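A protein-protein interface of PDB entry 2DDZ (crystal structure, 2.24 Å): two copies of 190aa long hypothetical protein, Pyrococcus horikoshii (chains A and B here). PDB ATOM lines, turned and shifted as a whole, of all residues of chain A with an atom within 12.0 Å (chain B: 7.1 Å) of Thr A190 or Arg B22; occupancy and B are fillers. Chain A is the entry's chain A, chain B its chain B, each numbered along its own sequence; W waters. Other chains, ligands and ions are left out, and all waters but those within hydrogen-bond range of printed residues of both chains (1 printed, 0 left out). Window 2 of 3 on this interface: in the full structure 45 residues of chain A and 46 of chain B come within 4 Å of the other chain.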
ATOM      1  N   VAL A 186     -39.889  10.402   4.789  1.00  0.00           N
ATOM      2  CA  VAL A 186     -38.519  10.658   4.377  1.00  0.00           C
ATOM      3  C   VAL A 186     -37.520  10.183   5.421  1.00  0.00           C
ATOM      4  O   VAL A 186     -37.748  10.321   6.630  1.00  0.00           O
ATOM      5  CB  VAL A 186     -38.280  12.182   4.149  1.00  0.00           C
ATOM      6  CG1 VAL A 186     -39.190  12.712   3.040  1.00  0.00           C
ATOM      7  CG2 VAL A 186     -38.535  12.936   5.449  1.00  0.00           C
ATOM      8  N   ARG A 187     -36.410   9.623   4.957  1.00  0.00           N
ATOM      9  CA  ARG A 187     -35.370   9.177   5.868  1.00  0.00           C
ATOM     10  C   ARG A 187     -34.454  10.374   6.150  1.00  0.00           C
ATOM     11  O   ARG A 187     -34.373  11.316   5.354  1.00  0.00           O
ATOM     12  CB  ARG A 187     -34.560   8.039   5.237  1.00  0.00           C
ATOM     13  CG  ARG A 187     -33.652   8.476   4.091  1.00  0.00           C
ATOM     14  CD  ARG A 187     -32.856   7.308   3.488  1.00  0.00           C
ATOM     15  NE  ARG A 187     -31.938   7.786   2.451  1.00  0.00           N
ATOM     16  CZ  ARG A 187     -30.737   8.315   2.689  1.00  0.00           C
ATOM     17  NH1 ARG A 187     -30.290   8.426   3.933  1.00  0.00           N
ATOM     18  NH2 ARG A 187     -29.986   8.746   1.681  1.00  0.00           N
ATOM     19  N   TRP A 188     -33.780  10.354   7.292  1.00  0.00           N
ATOM     20  CA  TRP A 188     -32.863  11.429   7.616  1.00  0.00           C
ATOM     21  C   TRP A 188     -31.617  11.184   6.782  1.00  0.00           C
ATOM     22  O   TRP A 188     -31.370  10.055   6.342  1.00  0.00           O
ATOM     23  CB  TRP A 188     -32.498  11.415   9.103  1.00  0.00           C
ATOM     24  CG  TRP A 188     -31.866  10.141   9.556  1.00  0.00           C
ATOM     25  CD1 TRP A 188     -32.501   8.964   9.837  1.00  0.00           C
ATOM     26  CD2 TRP A 188     -30.467   9.898   9.745  1.00  0.00           C
ATOM     27  NE1 TRP A 188     -31.582   8.001  10.189  1.00  0.00           N
ATOM     28  CE2 TRP A 188     -30.327   8.548  10.141  1.00  0.00           C
ATOM     29  CE3 TRP A 188     -29.317  10.688   9.619  1.00  0.00           C
ATOM     30  CZ2 TRP A 188     -29.082   7.972  10.408  1.00  0.00           C
ATOM     31  CZ3 TRP A 188     -28.079  10.114   9.885  1.00  0.00           C
ATOM     32  CH2 TRP A 188     -27.974   8.768  10.276  1.00  0.00           C
ATOM     33  N   VAL A 189     -30.835  12.239   6.572  1.00  0.00           N
ATOM     34  CA  VAL A 189     -29.622  12.142   5.784  1.00  0.00           C
ATOM     35  C   VAL A 189     -28.390  12.523   6.602  1.00  0.00           C
ATOM     36  O   VAL A 189     -28.505  13.203   7.621  1.00  0.00           O
ATOM     37  CB  VAL A 189     -29.706  13.057   4.556  1.00  0.00           C
ATOM     38  CG1 VAL A 189     -30.910  12.674   3.718  1.00  0.00           C
ATOM     39  CG2 VAL A 189     -29.782  14.509   4.991  1.00  0.00           C
ATOM     40  N   THR A 190     -27.213  12.084   6.148  1.00  0.00           N
ATOM     41  CA  THR A 190     -25.964  12.386   6.843  1.00  0.00           C
ATOM     42  C   THR A 190     -25.395  13.717   6.369  1.00  0.00           C
ATOM     43  O   THR A 190     -25.873  14.234   5.331  1.00  0.00           O
ATOM     44  CB  THR A 190     -24.900  11.283   6.612  1.00  0.00           C
ATOM     45  OG1 THR A 190     -24.560  11.236   5.222  1.00  0.00           O
ATOM     46  CG2 THR A 190     -25.428   9.910   7.047  1.00  0.00           C
ATOM     47  OXT THR A 190     -24.468  14.225   7.039  1.00  0.00           O
ATOM     48  N   TYR B  16     -26.838  15.825 -10.650  1.00  0.00           N
ATOM     49  CA  TYR B  16     -27.452  15.521  -9.369  1.00  0.00           C
ATOM     50  C   TYR B  16     -27.722  14.034  -9.263  1.00  0.00           C
ATOM     51  O   TYR B  16     -28.549  13.488  -9.994  1.00  0.00           O
ATOM     52  CB  TYR B  16     -28.774  16.290  -9.219  1.00  0.00           C
ATOM     53  CG  TYR B  16     -29.462  16.088  -7.883  1.00  0.00           C
ATOM     54  CD1 TYR B  16     -28.917  16.608  -6.708  1.00  0.00           C
ATOM     55  CD2 TYR B  16     -30.645  15.362  -7.791  1.00  0.00           C
ATOM     56  CE1 TYR B  16     -29.530  16.409  -5.479  1.00  0.00           C
ATOM     57  CE2 TYR B  16     -31.267  15.157  -6.561  1.00  0.00           C
ATOM     58  CZ  TYR B  16     -30.701  15.683  -5.411  1.00  0.00           C
ATOM     59  OH  TYR B  16     -31.295  15.476  -4.189  1.00  0.00           O
ATOM     60  N   GLY B  18     -28.191  12.797  -6.107  1.00  0.00           N
ATOM     61  CA  GLY B  18     -28.775  12.709  -4.777  1.00  0.00           C
ATOM     62  C   GLY B  18     -27.825  12.947  -3.610  1.00  0.00           C
ATOM     63  O   GLY B  18     -28.268  13.070  -2.467  1.00  0.00           O
ATOM     64  N   SER B  19     -26.524  13.020  -3.879  1.00  0.00           N
ATOM     65  CA  SER B  19     -25.557  13.228  -2.808  1.00  0.00           C
ATOM     66  C   SER B  19     -25.557  14.676  -2.311  1.00  0.00           C
ATOM     67  O   SER B  19     -25.162  14.943  -1.185  1.00  0.00           O
ATOM     68  CB  SER B  19     -24.147  12.834  -3.277  1.00  0.00           C
ATOM     69  OG  SER B  19     -23.627  13.777  -4.201  1.00  0.00           O
ATOM     70  N   ALA B  20     -26.004  15.608  -3.148  1.00  0.00           N
ATOM     71  CA  ALA B  20     -26.038  17.027  -2.772  1.00  0.00           C
ATOM     72  C   ALA B  20     -27.028  17.334  -1.635  1.00  0.00           C
ATOM     73  O   ALA B  20     -27.051  18.438  -1.104  1.00  0.00           O
ATOM     74  CB  ALA B  20     -26.381  17.880  -3.991  1.00  0.00           C
ATOM     75  N   ILE B  21     -27.826  16.348  -1.256  1.00  0.00           N
ATOM     76  CA  ILE B  21     -28.802  16.541  -0.213  1.00  0.00           C
ATOM     77  C   ILE B  21     -28.200  16.386   1.190  1.00  0.00           C
ATOM     78  O   ILE B  21     -28.846  16.724   2.184  1.00  0.00           O
ATOM     79  CB  ILE B  21     -29.920  15.516  -0.315  1.00  0.00           C
ATOM     80  CG1 ILE B  21     -31.127  16.029   0.464  1.00  0.00           C
ATOM     81  CG2 ILE B  21     -29.425  14.165   0.220  1.00  0.00           C
ATOM     82  CD1 ILE B  21     -32.375  15.251   0.177  1.00  0.00           C
ATOM     83  N   ARG B  22     -26.976  15.866   1.267  1.00  0.00           N
ATOM     84  CA  ARG B  22     -26.340  15.654   2.554  1.00  0.00           C
ATOM     85  C   ARG B  22     -25.888  16.921   3.273  1.00  0.00           C
ATOM     86  O   ARG B  22     -25.697  17.960   2.653  1.00  0.00           O
ATOM     87  CB  ARG B  22     -25.141  14.718   2.424  1.00  0.00           C
ATOM     88  CG  ARG B  22     -25.436  13.426   1.649  1.00  0.00           C
ATOM     89  CD  ARG B  22     -24.189  12.597   1.704  1.00  0.00           C
ATOM     90  NE  ARG B  22     -24.304  11.365   0.955  1.00  0.00           N
ATOM     91  CZ  ARG B  22     -23.961  10.188   1.444  1.00  0.00           C
ATOM     92  NH1 ARG B  22     -24.049   9.139   0.679  1.00  0.00           N
ATOM     93  NH2 ARG B  22     -23.551  10.076   2.702  1.00  0.00           N
ATOM     94  N   SER B  23     -25.676  16.833   4.587  1.00  0.00           N
ATOM     95  CA  SER B  23     -25.259  18.013   5.350  1.00  0.00           C
ATOM     96  C   SER B  23     -23.931  18.648   4.948  1.00  0.00           C
ATOM     97  O   SER B  23     -22.981  17.978   4.558  1.00  0.00           O
ATOM     98  CB  SER B  23     -25.227  17.681   6.837  1.00  0.00           C
ATOM     99  OG  SER B  23     -24.418  16.564   7.123  1.00  0.00           O
ATOM    100  N   HIS B  24     -23.883  19.968   5.070  1.00  0.00           N
ATOM    101  CA  HIS B  24     -22.695  20.765   4.758  1.00  0.00           C
ATOM    102  C   HIS B  24     -22.225  20.731   3.305  1.00  0.00           C
ATOM    103  O   HIS B  24     -21.178  21.307   2.968  1.00  0.00           O
ATOM    104  CB  HIS B  24     -21.545  20.352   5.685  1.00  0.00           C
ATOM    105  CG  HIS B  24     -21.723  20.806   7.105  1.00  0.00           C
ATOM    106  ND1 HIS B  24     -22.087  19.952   8.121  1.00  0.00           N
ATOM    107  CD2 HIS B  24     -21.565  22.026   7.676  1.00  0.00           C
ATOM    108  CE1 HIS B  24     -22.138  20.620   9.261  1.00  0.00           C
ATOM    109  NE2 HIS B  24     -21.824  21.880   9.017  1.00  0.00           N
ATOM    110  N   TRP B  25     -23.009  20.091   2.443  1.00  0.00           N
ATOM    111  CA  TRP B  25     -22.676  20.005   1.024  1.00  0.00           C
ATOM    112  C   TRP B  25     -22.176  21.336   0.466  1.00  0.00           C
ATOM    113  O   TRP B  25     -21.135  21.380  -0.187  1.00  0.00           O
ATOM    114  CB  TRP B  25     -23.896  19.544   0.209  1.00  0.00           C
ATOM    115  CG  TRP B  25     -23.645  19.415  -1.288  1.00  0.00           C
ATOM    116  CD1 TRP B  25     -23.030  18.379  -1.928  1.00  0.00           C
ATOM    117  CD2 TRP B  25     -23.981  20.371  -2.311  1.00  0.00           C
ATOM    118  NE1 TRP B  25     -22.957  18.627  -3.276  1.00  0.00           N
ATOM    119  CE2 TRP B  25     -23.531  19.842  -3.540  1.00  0.00           C
ATOM    120  CE3 TRP B  25     -24.610  21.620  -2.306  1.00  0.00           C
ATOM    121  CZ2 TRP B  25     -23.699  20.517  -4.755  1.00  0.00           C
ATOM    122  CZ3 TRP B  25     -24.776  22.294  -3.520  1.00  0.00           C
ATOM    123  CH2 TRP B  25     -24.319  21.738  -4.724  1.00  0.00           C
ATOM    124  N   ALA B  26     -22.905  22.421   0.723  1.00  0.00           N
ATOM    125  CA  ALA B  26     -22.503  23.719   0.185  1.00  0.00           C
ATOM    126  C   ALA B  26     -21.222  24.300   0.767  1.00  0.00           C
ATOM    127  O   ALA B  26     -20.416  24.889   0.042  1.00  0.00           O
ATOM    128  CB  ALA B  26     -23.645  24.743   0.329  1.00  0.00           C
ATOM    129  N   ARG B  28     -18.842  22.577   2.411  1.00  0.00           N
ATOM    130  CA  ARG B  28     -17.817  21.573   2.097  1.00  0.00           C
ATOM    131  C   ARG B  28     -17.251  21.668   0.682  1.00  0.00           C
ATOM    132  O   ARG B  28     -16.052  21.497   0.478  1.00  0.00           O
ATOM    133  CB  ARG B  28     -18.413  20.179   2.325  1.00  0.00           C
ATOM    134  CG  ARG B  28     -17.378  19.129   2.700  1.00  0.00           C
ATOM    135  CD  ARG B  28     -17.980  17.965   3.506  1.00  0.00           C
ATOM    136  NE  ARG B  28     -18.831  17.051   2.741  1.00  0.00           N
ATOM    137  CZ  ARG B  28     -20.140  17.210   2.542  1.00  0.00           C
ATOM    138  NH1 ARG B  28     -20.824  16.316   1.835  1.00  0.00           N
ATOM    139  NH2 ARG B  28     -20.770  18.262   3.046  1.00  0.00           N
ATOM    140  N   GLU B  49     -29.237   4.322  -3.319  1.00  0.00           N
ATOM    141  CA  GLU B  49     -28.676   4.366  -1.971  1.00  0.00           C
ATOM    142  C   GLU B  49     -28.748   5.805  -1.444  1.00  0.00           C
ATOM    143  O   GLU B  49     -28.550   6.048  -0.252  1.00  0.00           O
ATOM    144  CB  GLU B  49     -27.213   3.892  -1.962  1.00  0.00           C
ATOM    145  CG  GLU B  49     -26.247   4.781  -2.735  1.00  0.00           C
ATOM    146  CD  GLU B  49     -24.806   4.317  -2.615  1.00  0.00           C
ATOM    147  OE1 GLU B  49     -24.585   3.165  -2.177  1.00  0.00           O
ATOM    148  OE2 GLU B  49     -23.893   5.098  -2.968  1.00  0.00           O
ATOM    149  N   GLU B  50     -29.047   6.739  -2.350  1.00  0.00           N
ATOM    150  CA  GLU B  50     -29.145   8.163  -2.035  1.00  0.00           C
ATOM    151  C   GLU B  50     -30.582   8.719  -2.077  1.00  0.00           C
ATOM    152  O   GLU B  50     -30.792   9.936  -1.986  1.00  0.00           O
ATOM    153  CB  GLU B  50     -28.245   8.961  -2.986  1.00  0.00           C
ATOM    154  CG  GLU B  50     -26.756   8.658  -2.821  1.00  0.00           C
ATOM    155  CD  GLU B  50     -26.200   9.166  -1.500  1.00  0.00           C
ATOM    156  OE1 GLU B  50     -26.115  10.403  -1.321  1.00  0.00           O
ATOM    157  OE2 GLU B  50     -25.853   8.325  -0.641  1.00  0.00           O
ATOM    158  N   ILE B  72     -30.543  23.324  -4.076  1.00  0.00           N
ATOM    159  CA  ILE B  72     -30.108  22.676  -2.865  1.00  0.00           C
ATOM    160  C   ILE B  72     -30.100  23.718  -1.775  1.00  0.00           C
ATOM    161  O   ILE B  72     -29.354  24.694  -1.835  1.00  0.00           O
ATOM    162  CB  ILE B  72     -28.713  22.078  -3.022  1.00  0.00           C
ATOM    163  CG1 ILE B  72     -28.783  20.919  -4.023  1.00  0.00           C
ATOM    164  CG2 ILE B  72     -28.207  21.598  -1.677  1.00  0.00           C
ATOM    165  CD1 ILE B  72     -29.682  19.788  -3.580  1.00  0.00           C
ATOM    166  N   GLU B  74     -29.907  24.466   2.434  1.00  0.00           N
ATOM    167  CA  GLU B  74     -29.525  23.946   3.738  1.00  0.00           C
ATOM    168  C   GLU B  74     -29.741  25.039   4.764  1.00  0.00           C
ATOM    169  O   GLU B  74     -29.282  26.175   4.597  1.00  0.00           O
ATOM    170  CB  GLU B  74     -28.069  23.480   3.764  1.00  0.00           C
ATOM    171  CG  GLU B  74     -27.652  22.858   5.103  1.00  0.00           C
ATOM    172  CD  GLU B  74     -26.442  21.948   4.977  1.00  0.00           C
ATOM    173  OE1 GLU B  74     -25.578  22.239   4.130  1.00  0.00           O
ATOM    174  OE2 GLU B  74     -26.348  20.947   5.726  1.00  0.00           O
ATOM    175  N   VAL B 127     -34.081  16.073   7.053  1.00  0.00           N
ATOM    176  CA  VAL B 127     -33.154  16.661   8.005  1.00  0.00           C
ATOM    177  C   VAL B 127     -31.936  15.779   8.234  1.00  0.00           C
ATOM    178  O   VAL B 127     -31.977  14.559   7.998  1.00  0.00           O
ATOM    179  CB  VAL B 127     -33.834  16.885   9.383  1.00  0.00           C
ATOM    180  CG1 VAL B 127     -34.982  17.875   9.256  1.00  0.00           C
ATOM    181  CG2 VAL B 127     -34.351  15.551   9.927  1.00  0.00           C
ATOM    182  N   SER B 128     -30.863  16.421   8.695  1.00  0.00           N
ATOM    183  CA  SER B 128     -29.613  15.754   9.044  1.00  0.00           C
ATOM    184  C   SER B 128     -29.519  15.987  10.544  1.00  0.00           C
ATOM    185  O   SER B 128     -30.343  16.707  11.112  1.00  0.00           O
ATOM    186  CB  SER B 128     -28.415  16.399   8.337  1.00  0.00           C
ATOM    187  OG  SER B 128     -28.099  17.667   8.874  1.00  0.00           O
ATOM    188  N   PRO B 129     -28.543  15.369  11.220  1.00  0.00           N
ATOM    189  CA  PRO B 129     -28.480  15.616  12.666  1.00  0.00           C
ATOM    190  C   PRO B 129     -28.225  17.088  13.029  1.00  0.00           C
ATOM    191  O   PRO B 129     -28.418  17.489  14.172  1.00  0.00           O
ATOM    192  CB  PRO B 129     -27.335  14.705  13.122  1.00  0.00           C
ATOM    193  CG  PRO B 129     -27.393  13.565  12.130  1.00  0.00           C
ATOM    194  CD  PRO B 129     -27.628  14.281  10.820  1.00  0.00           C
ATOM    195  N   VAL B 130     -27.811  17.895  12.058  1.00  0.00           N
ATOM    196  CA  VAL B 130     -27.499  19.291  12.349  1.00  0.00           C
ATOM    197  C   VAL B 130     -28.119  20.315  11.423  1.00  0.00           C
ATOM    198  O   VAL B 130     -27.778  21.500  11.498  1.00  0.00           O
ATOM    199  CB  VAL B 130     -25.974  19.540  12.306  1.00  0.00           C
ATOM    200  CG1 VAL B 130     -25.270  18.606  13.270  1.00  0.00           C
ATOM    201  CG2 VAL B 130     -25.455  19.349  10.878  1.00  0.00           C
ATOM    202  N   SER B 131     -29.021  19.887  10.550  1.00  0.00           N
ATOM    203  CA  SER B 131     -29.603  20.846   9.619  1.00  0.00           C
ATOM    204  C   SER B 131     -30.823  20.366   8.865  1.00  0.00           C
ATOM    205  O   SER B 131     -31.197  19.188   8.891  1.00  0.00           O
ATOM    206  CB  SER B 131     -28.556  21.239   8.582  1.00  0.00           C
ATOM    207  OG  SER B 131     -28.231  20.107   7.775  1.00  0.00           O
ATOM    208  N   LYS B 133     -32.524  20.093   5.062  1.00  0.00           N
ATOM    209  CA  LYS B 133     -32.092  20.053   3.676  1.00  0.00           C
ATOM    210  C   LYS B 133     -33.218  19.781   2.718  1.00  0.00           C
ATOM    211  O   LYS B 133     -33.953  18.817   2.864  1.00  0.00           O
ATOM    212  CB  LYS B 133     -30.980  19.017   3.478  1.00  0.00           C
ATOM    213  CG  LYS B 133     -29.659  19.470   4.109  1.00  0.00           C
ATOM    214  CD  LYS B 133     -28.448  19.248   3.202  1.00  0.00           C
ATOM    215  CE  LYS B 133     -28.623  19.843   1.806  1.00  0.00           C
ATOM    216  NZ  LYS B 133     -27.319  19.928   1.083  1.00  0.00           N
HETATM  217  O   HOH W   1     -22.697  15.507   5.078  1.00  0.00           O
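The backbone NH of Val A189 sits at hydrogen-bond distance from the backbone carbonyl oxygen of Val B127, 3.0 Å away. The side-chain hydroxyl (OG1) of Thr A190 lies within hydrogen-bond range of the guanidinium group (NH2) of Arg B22, 3.0 Å away. N of Ser B23 lies within hydrogen-bond range of O of Thr A190 (2.7 Å).
Among the printed residues, merely in contact across the chains: Arg A187 with Glu B49 (3.6 Å), Arg A187 with Glu B50 (3.8 Å), Trp A188 with Val B127 (3.3 Å), Val A189 with Ile B21 (3.7 Å), Val A189 with Ser B128 (3.1 Å) and Val A189 with Pro B129 (3.5 Å).
Of the printed residues of chain B, Trp A188 touches Val B127 (3.3 Å). Of the printed residues of chain B, Val A189 touches Ile B21, Val B127, Ser B128 and Pro B129. Thr A190 touches just these residues of chain B: Arg B22 (3.0 Å) and Ser B23 (2.3 Å). Gly B18 touches none of the printed residues of chain A. No residue of chain A comes within 4 Å of Ser B19. Ala B20 touches none of the printed residues of chain A. Of chain A, only Val A189 comes within 4 Å of Ile B21. Arg B22 touches just one residue of chain A: Thr A190 (3.0 Å). Of chain A, only Thr A190 comes within 4 Å of Ser B23. Of the printed residues of chain A, Glu B49 touches Arg A187 (3.6 Å). Of chain A, only Arg A187 (3.8 Å) comes within 4 Å of Glu B50. Of the printed residues of chain A, Val B127 touches Trp A188 and Val A189. Ser B128 touches just one residue of chain A: Val A189 (3.1 Å). Of the printed residues of chain A, Pro B129 touches Val A189. The nearest residue of chain A that does not touch Arg B22 is Val A189 (4.4 Å).
Water W1 lies within hydrogen-bond range of O of Ser B23 (2.5 Å) and OXT of Thr A190 (2.9 Å).
No position is printed for both chains. Of the 9 pairs that touch across the chains among the printed residues, none has its exchanged pair printed and touching as well.
NE of Arg B22 lies within salt-bridge range of OE1 of Glu B50 (3.1 Å). The side-chain amino group of Lys B133 lies within hydrogen-bond range of the backbone carbonyl oxygen of Arg B22. The backbone carbonyl oxygen of Ser B23 is in hydrogen-bond range of the guanidinium group of Arg B28 (2.7 Å). The side-chain hydroxyl (OG) of Ser B128 lies close to the backbone NH (N) of Val B130 (3.2 Å). The side-chain hydroxyl (OG) of Ser B131 is in hydrogen-bond range of the side-chain hydroxyl (OG) of Ser B128 (2.7 Å).
Hydrophobic or aromatic side chains of chain B that line the printed part of chain A: Pro B129. Among the printed residues, no Asp or Glu carboxylate lies within 4 Å of a Lys or Arg side-chain nitrogen of the other chain.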
